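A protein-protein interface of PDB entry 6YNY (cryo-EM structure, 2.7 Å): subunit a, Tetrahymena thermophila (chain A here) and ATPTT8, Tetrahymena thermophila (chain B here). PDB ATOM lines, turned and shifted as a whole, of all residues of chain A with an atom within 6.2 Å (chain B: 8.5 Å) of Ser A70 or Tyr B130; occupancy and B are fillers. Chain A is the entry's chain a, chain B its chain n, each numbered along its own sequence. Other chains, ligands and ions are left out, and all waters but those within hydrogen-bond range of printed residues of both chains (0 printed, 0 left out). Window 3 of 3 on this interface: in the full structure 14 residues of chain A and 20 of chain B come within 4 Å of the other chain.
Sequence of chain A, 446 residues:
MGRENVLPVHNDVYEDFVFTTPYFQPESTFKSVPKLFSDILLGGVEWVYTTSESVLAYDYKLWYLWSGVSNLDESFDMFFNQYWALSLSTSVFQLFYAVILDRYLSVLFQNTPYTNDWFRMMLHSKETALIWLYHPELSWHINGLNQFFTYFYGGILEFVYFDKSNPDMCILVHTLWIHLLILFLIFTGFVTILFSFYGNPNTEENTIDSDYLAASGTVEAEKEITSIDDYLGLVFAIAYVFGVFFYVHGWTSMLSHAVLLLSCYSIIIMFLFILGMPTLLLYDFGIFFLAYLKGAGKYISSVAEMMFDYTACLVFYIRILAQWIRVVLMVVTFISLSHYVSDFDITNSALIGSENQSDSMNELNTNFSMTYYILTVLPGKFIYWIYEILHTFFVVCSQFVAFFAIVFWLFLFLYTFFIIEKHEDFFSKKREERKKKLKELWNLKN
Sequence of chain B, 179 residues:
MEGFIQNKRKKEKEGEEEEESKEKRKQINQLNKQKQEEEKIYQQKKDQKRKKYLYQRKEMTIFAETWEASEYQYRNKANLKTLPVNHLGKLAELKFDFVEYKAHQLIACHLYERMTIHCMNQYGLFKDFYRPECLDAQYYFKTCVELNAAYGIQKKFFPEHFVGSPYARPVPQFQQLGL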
ATOM      1  N   SER A  67     -11.079  19.080 -12.659  1.00  0.00           N
ATOM      2  CA  SER A  67     -11.974  19.804 -11.767  1.00  0.00           C
ATOM      3  C   SER A  67     -11.303  20.114 -10.439  1.00  0.00           C
ATOM      4  O   SER A  67     -11.531  21.179  -9.854  1.00  0.00           O
ATOM      5  CB  SER A  67     -13.248  18.994 -11.544  1.00  0.00           C
ATOM      6  OG  SER A  67     -12.949  17.727 -10.987  1.00  0.00           O
ATOM      7  N   GLY A  68     -10.464  19.206  -9.952  1.00  0.00           N
ATOM      8  CA  GLY A  68      -9.843  19.367  -8.661  1.00  0.00           C
ATOM      9  C   GLY A  68     -10.737  19.067  -7.482  1.00  0.00           C
ATOM     10  O   GLY A  68     -10.289  19.204  -6.337  1.00  0.00           O
ATOM     11  N   VAL A  69     -11.985  18.661  -7.719  1.00  0.00           N
ATOM     12  CA  VAL A  69     -12.945  18.395  -6.660  1.00  0.00           C
ATOM     13  C   VAL A  69     -13.441  16.956  -6.681  1.00  0.00           C
ATOM     14  O   VAL A  69     -14.388  16.623  -5.969  1.00  0.00           O
ATOM     15  CB  VAL A  69     -14.132  19.376  -6.733  1.00  0.00           C
ATOM     16  CG1 VAL A  69     -13.634  20.801  -6.729  1.00  0.00           C
ATOM     17  CG2 VAL A  69     -14.972  19.112  -7.959  1.00  0.00           C
ATOM     18  N   SER A  70     -12.825  16.094  -7.480  1.00  0.00           N
ATOM     19  CA  SER A  70     -13.218  14.696  -7.586  1.00  0.00           C
ATOM     20  C   SER A  70     -12.106  13.819  -7.034  1.00  0.00           C
ATOM     21  O   SER A  70     -10.990  13.820  -7.565  1.00  0.00           O
ATOM     22  CB  SER A  70     -13.519  14.323  -9.034  1.00  0.00           C
ATOM     23  OG  SER A  70     -13.849  12.955  -9.155  1.00  0.00           O
ATOM     24  N   ASN A  71     -12.413  13.072  -5.978  1.00  0.00           N
ATOM     25  CA  ASN A  71     -11.471  12.129  -5.396  1.00  0.00           C
ATOM     26  C   ASN A  71     -11.407  10.811  -6.154  1.00  0.00           C
ATOM     27  O   ASN A  71     -10.678   9.909  -5.732  1.00  0.00           O
ATOM     28  CB  ASN A  71     -11.835  11.858  -3.936  1.00  0.00           C
ATOM     29  CG  ASN A  71     -13.235  11.301  -3.772  1.00  0.00           C
ATOM     30  OD1 ASN A  71     -13.860  10.856  -4.734  1.00  0.00           O
ATOM     31  ND2 ASN A  71     -13.736  11.327  -2.548  1.00  0.00           N
ATOM     32  N   LEU A  72     -12.145  10.678  -7.253  1.00  0.00           N
ATOM     33  CA  LEU A  72     -12.152   9.447  -8.026  1.00  0.00           C
ATOM     34  C   LEU A  72     -11.021   9.373  -9.037  1.00  0.00           C
ATOM     35  O   LEU A  72     -10.652   8.269  -9.452  1.00  0.00           O
ATOM     36  CB  LEU A  72     -13.479   9.297  -8.769  1.00  0.00           C
ATOM     37  CG  LEU A  72     -14.767   9.473  -7.966  1.00  0.00           C
ATOM     38  CD1 LEU A  72     -15.960   9.265  -8.863  1.00  0.00           C
ATOM     39  CD2 LEU A  72     -14.825   8.522  -6.800  1.00  0.00           C
ATOM     40  N   ASP A  73     -10.471  10.507  -9.445  1.00  0.00           N
ATOM     41  CA  ASP A  73      -9.437  10.572 -10.464  1.00  0.00           C
ATOM     42  C   ASP A  73      -8.184  11.219  -9.887  1.00  0.00           C
ATOM     43  O   ASP A  73      -8.123  11.570  -8.706  1.00  0.00           O
ATOM     44  CB  ASP A  73      -9.939  11.335 -11.693  1.00  0.00           C
ATOM     45  CG  ASP A  73     -10.327  12.763 -11.378  1.00  0.00           C
ATOM     46  OD1 ASP A  73     -10.290  13.146 -10.191  1.00  0.00           O
ATOM     47  OD2 ASP A  73     -10.670  13.504 -12.322  1.00  0.00           O
ATOM     48  N   GLU A  74      -7.176  11.378 -10.738  1.00  0.00           N
ATOM     49  CA  GLU A  74      -5.885  11.909 -10.330  1.00  0.00           C
ATOM     50  C   GLU A  74      -5.821  13.431 -10.353  1.00  0.00           C
ATOM     51  O   GLU A  74      -4.755  13.991 -10.085  1.00  0.00           O
ATOM     52  CB  GLU A  74      -4.781  11.343 -11.222  1.00  0.00           C
ATOM     53  CG  GLU A  74      -4.645   9.840 -11.166  1.00  0.00           C
ATOM     54  CD  GLU A  74      -3.395   9.339 -11.859  1.00  0.00           C
ATOM     55  OE1 GLU A  74      -2.365  10.040 -11.806  1.00  0.00           O
ATOM     56  OE2 GLU A  74      -3.442   8.250 -12.464  1.00  0.00           O
ATOM     57  N   SER A  75      -6.922  14.114 -10.667  1.00  0.00           N
ATOM     58  CA  SER A  75      -6.933  15.570 -10.640  1.00  0.00           C
ATOM     59  C   SER A  75      -7.078  16.128  -9.232  1.00  0.00           C
ATOM     60  O   SER A  75      -6.924  17.339  -9.045  1.00  0.00           O
ATOM     61  CB  SER A  75      -8.065  16.114 -11.513  1.00  0.00           C
ATOM     62  OG  SER A  75      -9.331  15.871 -10.926  1.00  0.00           O
ATOM     63  N   PHE A  76      -7.369  15.283  -8.249  1.00  0.00           N
ATOM     64  CA  PHE A  76      -7.532  15.737  -6.876  1.00  0.00           C
ATOM     65  C   PHE A  76      -6.183  16.137  -6.297  1.00  0.00           C
ATOM     66  O   PHE A  76      -5.269  15.312  -6.205  1.00  0.00           O
ATOM     67  CB  PHE A  76      -8.169  14.632  -6.040  1.00  0.00           C
ATOM     68  CG  PHE A  76      -8.607  15.075  -4.681  1.00  0.00           C
ATOM     69  CD1 PHE A  76      -9.766  15.810  -4.519  1.00  0.00           C
ATOM     70  CD2 PHE A  76      -7.872  14.744  -3.563  1.00  0.00           C
ATOM     71  CE1 PHE A  76     -10.173  16.212  -3.273  1.00  0.00           C
ATOM     72  CE2 PHE A  76      -8.277  15.147  -2.311  1.00  0.00           C
ATOM     73  CZ  PHE A  76      -9.428  15.879  -2.167  1.00  0.00           C
ATOM     74  N   CYS B 119     -19.253  23.235   4.484  1.00  0.00           N
ATOM     75  CA  CYS B 119     -19.723  22.049   3.781  1.00  0.00           C
ATOM     76  C   CYS B 119     -18.953  20.804   4.196  1.00  0.00           C
ATOM     77  O   CYS B 119     -19.522  19.708   4.225  1.00  0.00           O
ATOM     78  CB  CYS B 119     -19.622  22.263   2.272  1.00  0.00           C
ATOM     79  SG  CYS B 119     -20.660  23.591   1.634  1.00  0.00           S
ATOM     80  N   TYR B 123     -21.320  18.019   5.959  1.00  0.00           N
ATOM     81  CA  TYR B 123     -21.028  16.779   5.271  1.00  0.00           C
ATOM     82  C   TYR B 123     -19.549  16.460   5.452  1.00  0.00           C
ATOM     83  O   TYR B 123     -18.806  17.192   6.105  1.00  0.00           O
ATOM     84  CB  TYR B 123     -21.402  16.886   3.795  1.00  0.00           C
ATOM     85  CG  TYR B 123     -22.640  17.706   3.540  1.00  0.00           C
ATOM     86  CD1 TYR B 123     -22.542  19.009   3.089  1.00  0.00           C
ATOM     87  CD2 TYR B 123     -23.902  17.185   3.759  1.00  0.00           C
ATOM     88  CE1 TYR B 123     -23.663  19.766   2.857  1.00  0.00           C
ATOM     89  CE2 TYR B 123     -25.029  17.936   3.532  1.00  0.00           C
ATOM     90  CZ  TYR B 123     -24.906  19.227   3.080  1.00  0.00           C
ATOM     91  OH  TYR B 123     -26.030  19.981   2.850  1.00  0.00           O
ATOM     92  N   GLY B 124     -19.117  15.349   4.874  1.00  0.00           N
ATOM     93  CA  GLY B 124     -17.727  14.955   4.971  1.00  0.00           C
ATOM     94  C   GLY B 124     -16.966  15.171   3.682  1.00  0.00           C
ATOM     95  O   GLY B 124     -16.946  16.275   3.134  1.00  0.00           O
ATOM     96  N   LEU B 125     -16.314  14.111   3.206  1.00  0.00           N
ATOM     97  CA  LEU B 125     -15.606  14.123   1.935  1.00  0.00           C
ATOM     98  C   LEU B 125     -16.003  12.943   1.057  1.00  0.00           C
ATOM     99  O   LEU B 125     -15.349  12.700   0.037  1.00  0.00           O
ATOM    100  CB  LEU B 125     -14.088  14.103   2.161  1.00  0.00           C
ATOM    101  CG  LEU B 125     -13.357  15.381   2.578  1.00  0.00           C
ATOM    102  CD1 LEU B 125     -13.433  16.431   1.496  1.00  0.00           C
ATOM    103  CD2 LEU B 125     -13.901  15.925   3.879  1.00  0.00           C
ATOM    104  N   PHE B 126     -17.054  12.206   1.419  1.00  0.00           N
ATOM    105  CA  PHE B 126     -17.408  10.962   0.742  1.00  0.00           C
ATOM    106  C   PHE B 126     -18.922  10.860   0.618  1.00  0.00           C
ATOM    107  O   PHE B 126     -19.616  10.683   1.623  1.00  0.00           O
ATOM    108  CB  PHE B 126     -16.867   9.747   1.494  1.00  0.00           C
ATOM    109  CG  PHE B 126     -15.453   9.895   1.959  1.00  0.00           C
ATOM    110  CD1 PHE B 126     -14.396   9.617   1.115  1.00  0.00           C
ATOM    111  CD2 PHE B 126     -15.180  10.296   3.250  1.00  0.00           C
ATOM    112  CE1 PHE B 126     -13.099   9.747   1.548  1.00  0.00           C
ATOM    113  CE2 PHE B 126     -13.884  10.426   3.688  1.00  0.00           C
ATOM    114  CZ  PHE B 126     -12.842  10.152   2.837  1.00  0.00           C
ATOM    115  N   LYS B 127     -19.436  10.976  -0.604  1.00  0.00           N
ATOM    116  CA  LYS B 127     -20.803  10.614  -0.970  1.00  0.00           C
ATOM    117  C   LYS B 127     -21.847  11.558  -0.392  1.00  0.00           C
ATOM    118  O   LYS B 127     -23.032  11.417  -0.710  1.00  0.00           O
ATOM    119  CB  LYS B 127     -21.144   9.182  -0.539  1.00  0.00           C
ATOM    120  CG  LYS B 127     -22.392   8.604  -1.187  1.00  0.00           C
ATOM    121  CD  LYS B 127     -22.646   7.173  -0.744  1.00  0.00           C
ATOM    122  CE  LYS B 127     -23.081   7.103   0.712  1.00  0.00           C
ATOM    123  NZ  LYS B 127     -23.426   5.715   1.133  1.00  0.00           N
ATOM    124  N   ASP B 128     -21.452  12.523   0.424  1.00  0.00           N
ATOM    125  CA  ASP B 128     -22.342  13.551   0.936  1.00  0.00           C
ATOM    126  C   ASP B 128     -21.871  14.949   0.599  1.00  0.00           C
ATOM    127  O   ASP B 128     -22.700  15.845   0.431  1.00  0.00           O
ATOM    128  CB  ASP B 128     -22.490  13.428   2.458  1.00  0.00           C
ATOM    129  CG  ASP B 128     -23.187  12.152   2.876  1.00  0.00           C
ATOM    130  OD1 ASP B 128     -23.625  11.392   1.987  1.00  0.00           O
ATOM    131  OD2 ASP B 128     -23.297  11.907   4.095  1.00  0.00           O
ATOM    132  N   PHE B 129     -20.562  15.157   0.500  1.00  0.00           N
ATOM    133  CA  PHE B 129     -20.017  16.425   0.052  1.00  0.00           C
ATOM    134  C   PHE B 129     -20.147  16.602  -1.451  1.00  0.00           C
ATOM    135  O   PHE B 129     -20.041  17.731  -1.941  1.00  0.00           O
ATOM    136  CB  PHE B 129     -18.550  16.508   0.464  1.00  0.00           C
ATOM    137  CG  PHE B 129     -17.880  17.783   0.084  1.00  0.00           C
ATOM    138  CD1 PHE B 129     -18.051  18.920   0.840  1.00  0.00           C
ATOM    139  CD2 PHE B 129     -17.055  17.837  -1.018  1.00  0.00           C
ATOM    140  CE1 PHE B 129     -17.426  20.091   0.495  1.00  0.00           C
ATOM    141  CE2 PHE B 129     -16.430  19.004  -1.366  1.00  0.00           C
ATOM    142  CZ  PHE B 129     -16.615  20.133  -0.608  1.00  0.00           C
ATOM    143  N   TYR B 130     -20.390  15.518  -2.186  1.00  0.00           N
ATOM    144  CA  TYR B 130     -20.478  15.567  -3.641  1.00  0.00           C
ATOM    145  C   TYR B 130     -21.893  15.974  -4.046  1.00  0.00           C
ATOM    146  O   TYR B 130     -22.684  15.199  -4.586  1.00  0.00           O
ATOM    147  CB  TYR B 130     -20.060  14.236  -4.243  1.00  0.00           C
ATOM    148  CG  TYR B 130     -18.565  14.096  -4.332  1.00  0.00           C
ATOM    149  CD1 TYR B 130     -17.896  14.387  -5.507  1.00  0.00           C
ATOM    150  CD2 TYR B 130     -17.819  13.705  -3.236  1.00  0.00           C
ATOM    151  CE1 TYR B 130     -16.532  14.276  -5.592  1.00  0.00           C
ATOM    152  CE2 TYR B 130     -16.455  13.593  -3.313  1.00  0.00           C
ATOM    153  CZ  TYR B 130     -15.814  13.880  -4.492  1.00  0.00           C
ATOM    154  OH  TYR B 130     -14.449  13.769  -4.575  1.00  0.00           O
ATOM    155  N   ARG B 131     -22.196  17.233  -3.768  1.00  0.00           N
ATOM    156  CA  ARG B 131     -23.422  17.894  -4.172  1.00  0.00           C
ATOM    157  C   ARG B 131     -23.070  19.250  -4.762  1.00  0.00           C
ATOM    158  O   ARG B 131     -22.052  19.843  -4.396  1.00  0.00           O
ATOM    159  CB  ARG B 131     -24.375  18.057  -2.980  1.00  0.00           C
ATOM    160  CG  ARG B 131     -23.839  18.917  -1.875  1.00  0.00           C
ATOM    161  CD  ARG B 131     -24.455  18.574  -0.537  1.00  0.00           C
ATOM    162  NE  ARG B 131     -25.913  18.559  -0.569  1.00  0.00           N
ATOM    163  CZ  ARG B 131     -26.672  17.536  -0.184  1.00  0.00           C
ATOM    164  NH1 ARG B 131     -26.133  16.421   0.284  1.00  0.00           N
ATOM    165  NH2 ARG B 131     -27.989  17.638  -0.261  1.00  0.00           N
ATOM    166  N   PRO B 132     -23.889  19.764  -5.681  1.00  0.00           N
ATOM    167  CA  PRO B 132     -23.436  20.909  -6.487  1.00  0.00           C
ATOM    168  C   PRO B 132     -23.109  22.147  -5.675  1.00  0.00           C
ATOM    169  O   PRO B 132     -22.181  22.883  -6.031  1.00  0.00           O
ATOM    170  CB  PRO B 132     -24.615  21.142  -7.441  1.00  0.00           C
ATOM    171  CG  PRO B 132     -25.777  20.577  -6.753  1.00  0.00           C
ATOM    172  CD  PRO B 132     -25.285  19.408  -5.974  1.00  0.00           C
ATOM    173  N   GLU B 133     -23.841  22.405  -4.593  1.00  0.00           N
ATOM    174  CA  GLU B 133     -23.593  23.612  -3.815  1.00  0.00           C
ATOM    175  C   GLU B 133     -22.235  23.577  -3.130  1.00  0.00           C
ATOM    176  O   GLU B 133     -21.619  24.629  -2.931  1.00  0.00           O
ATOM    177  CB  GLU B 133     -24.697  23.818  -2.778  1.00  0.00           C
ATOM    178  CG  GLU B 133     -24.979  22.617  -1.894  1.00  0.00           C
ATOM    179  CD  GLU B 133     -26.061  21.714  -2.455  1.00  0.00           C
ATOM    180  OE1 GLU B 133     -26.458  21.908  -3.622  1.00  0.00           O
ATOM    181  OE2 GLU B 133     -26.515  20.810  -1.725  1.00  0.00           O
ATOM    182  N   CYS B 134     -21.751  22.392  -2.771  1.00  0.00           N
ATOM    183  CA  CYS B 134     -20.499  22.277  -2.038  1.00  0.00           C
ATOM    184  C   CYS B 134     -19.291  22.122  -2.951  1.00  0.00           C
ATOM    185  O   CYS B 134     -18.204  22.596  -2.607  1.00  0.00           O
ATOM    186  CB  CYS B 134     -20.564  21.088  -1.077  1.00  0.00           C
ATOM    187  SG  CYS B 134     -22.084  20.982  -0.126  1.00  0.00           S
ATOM    188  N   LEU B 135     -19.451  21.463  -4.099  1.00  0.00           N
ATOM    189  CA  LEU B 135     -18.327  21.299  -5.012  1.00  0.00           C
ATOM    190  C   LEU B 135     -17.997  22.595  -5.738  1.00  0.00           C
ATOM    191  O   LEU B 135     -16.831  22.838  -6.063  1.00  0.00           O
ATOM    192  CB  LEU B 135     -18.622  20.193  -6.019  1.00  0.00           C
ATOM    193  CG  LEU B 135     -18.728  18.776  -5.466  1.00  0.00           C
ATOM    194  CD1 LEU B 135     -19.101  17.825  -6.566  1.00  0.00           C
ATOM    195  CD2 LEU B 135     -17.434  18.339  -4.822  1.00  0.00           C
ATOM    196  N   ASP B 136     -18.999  23.428  -6.013  1.00  0.00           N
ATOM    197  CA  ASP B 136     -18.726  24.707  -6.656  1.00  0.00           C
ATOM    198  C   ASP B 136     -17.980  25.649  -5.724  1.00  0.00           C
ATOM    199  O   ASP B 136     -17.176  26.466  -6.185  1.00  0.00           O
ATOM    200  CB  ASP B 136     -20.023  25.350  -7.131  1.00  0.00           C
ATOM    201  CG  ASP B 136     -20.608  24.661  -8.345  1.00  0.00           C
ATOM    202  OD1 ASP B 136     -20.133  23.561  -8.696  1.00  0.00           O
ATOM    203  OD2 ASP B 136     -21.539  25.225  -8.955  1.00  0.00           O
ATOM    204  N   GLN B 138     -15.791  24.634  -3.413  1.00  0.00           N
ATOM    205  CA  GLN B 138     -14.426  24.133  -3.421  1.00  0.00           C
ATOM    206  C   GLN B 138     -13.710  24.503  -4.712  1.00  0.00           C
ATOM    207  O   GLN B 138     -12.507  24.783  -4.704  1.00  0.00           O
ATOM    208  CB  GLN B 138     -14.440  22.620  -3.227  1.00  0.00           C
ATOM    209  CG  GLN B 138     -13.088  22.003  -2.995  1.00  0.00           C
ATOM    210  CD  GLN B 138     -13.137  20.495  -3.010  1.00  0.00           C
ATOM    211  OE1 GLN B 138     -14.134  19.900  -3.412  1.00  0.00           O
ATOM    212  NE2 GLN B 138     -12.059  19.866  -2.572  1.00  0.00           N
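Of the 10 printed residues of chain A, 3 touch a printed residue of chain B. Printed residues of chain A that touch a printed residue of chain B: Val A69, Ser A70 and Asn A71. Hydrophobic or aromatic side chains of chain B within 4 Å of the printed part of chain A: Tyr B130 and Leu B135. Among the printed residues, 6 pairs touch across the chains. Among the printed residues, no Asp or Glu carboxylate lies within 4 Å of a Lys or Arg side-chain nitrogen of the other chain.
The side-chain hydroxyl (OH) of Tyr B130 lies within hydrogen-bond range of the backbone carbonyl oxygen (O) of Val A69. The side-chain amide nitrogen of Asn A71 lies within hydrogen-bond range of the backbone carbonyl oxygen of Leu B125. The backbone NH of Asn A71 is in hydrogen-bond range of the side-chain hydroxyl of Tyr B130 (2.6 Å).
Among the printed residues, merely in contact across the chains: Val A69 with Leu B135 (3.7 Å), Val A69 with Gln B138 (3.4 Å) and Ser A70 with Tyr B130 (3.4 Å).
The backbone NH (N) of Leu A72 lies close to the side-chain hydroxyl (OG) of Ser A70 (3.4 Å).
Of chain B, only Tyr B130 comes within 4 Å of Ser A70. Tyr B130 touches just these residues of chain A: Val A69 (3.2 Å), Ser A70 (3.4 Å) and Asn A71 (2.6 Å). Asn A71 touches just these residues of chain B: Leu B125 and Tyr B130. Printed residues of chain A within 4 Å of Gln B138: Val A69 (3.4 Å). Of the printed residues of chain B, Val A69 touches Tyr B130, Leu B135 and Gln B138. Of the printed residues of chain A, Leu B125 touches Asn A71. Phe A76 touches none of the printed residues of chain B. Ser A75 touches none of the printed residues of chain B. The nearest residue of chain B that does not touch Ser A70 is Gln B138 (5.7 Å). The nearest residue of chain A that does not touch Tyr B130 is Leu A72 (4.7 Å). The nearest printed residue of chain A that does not touch Leu B135 is Ser A70 (5.8 Å).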
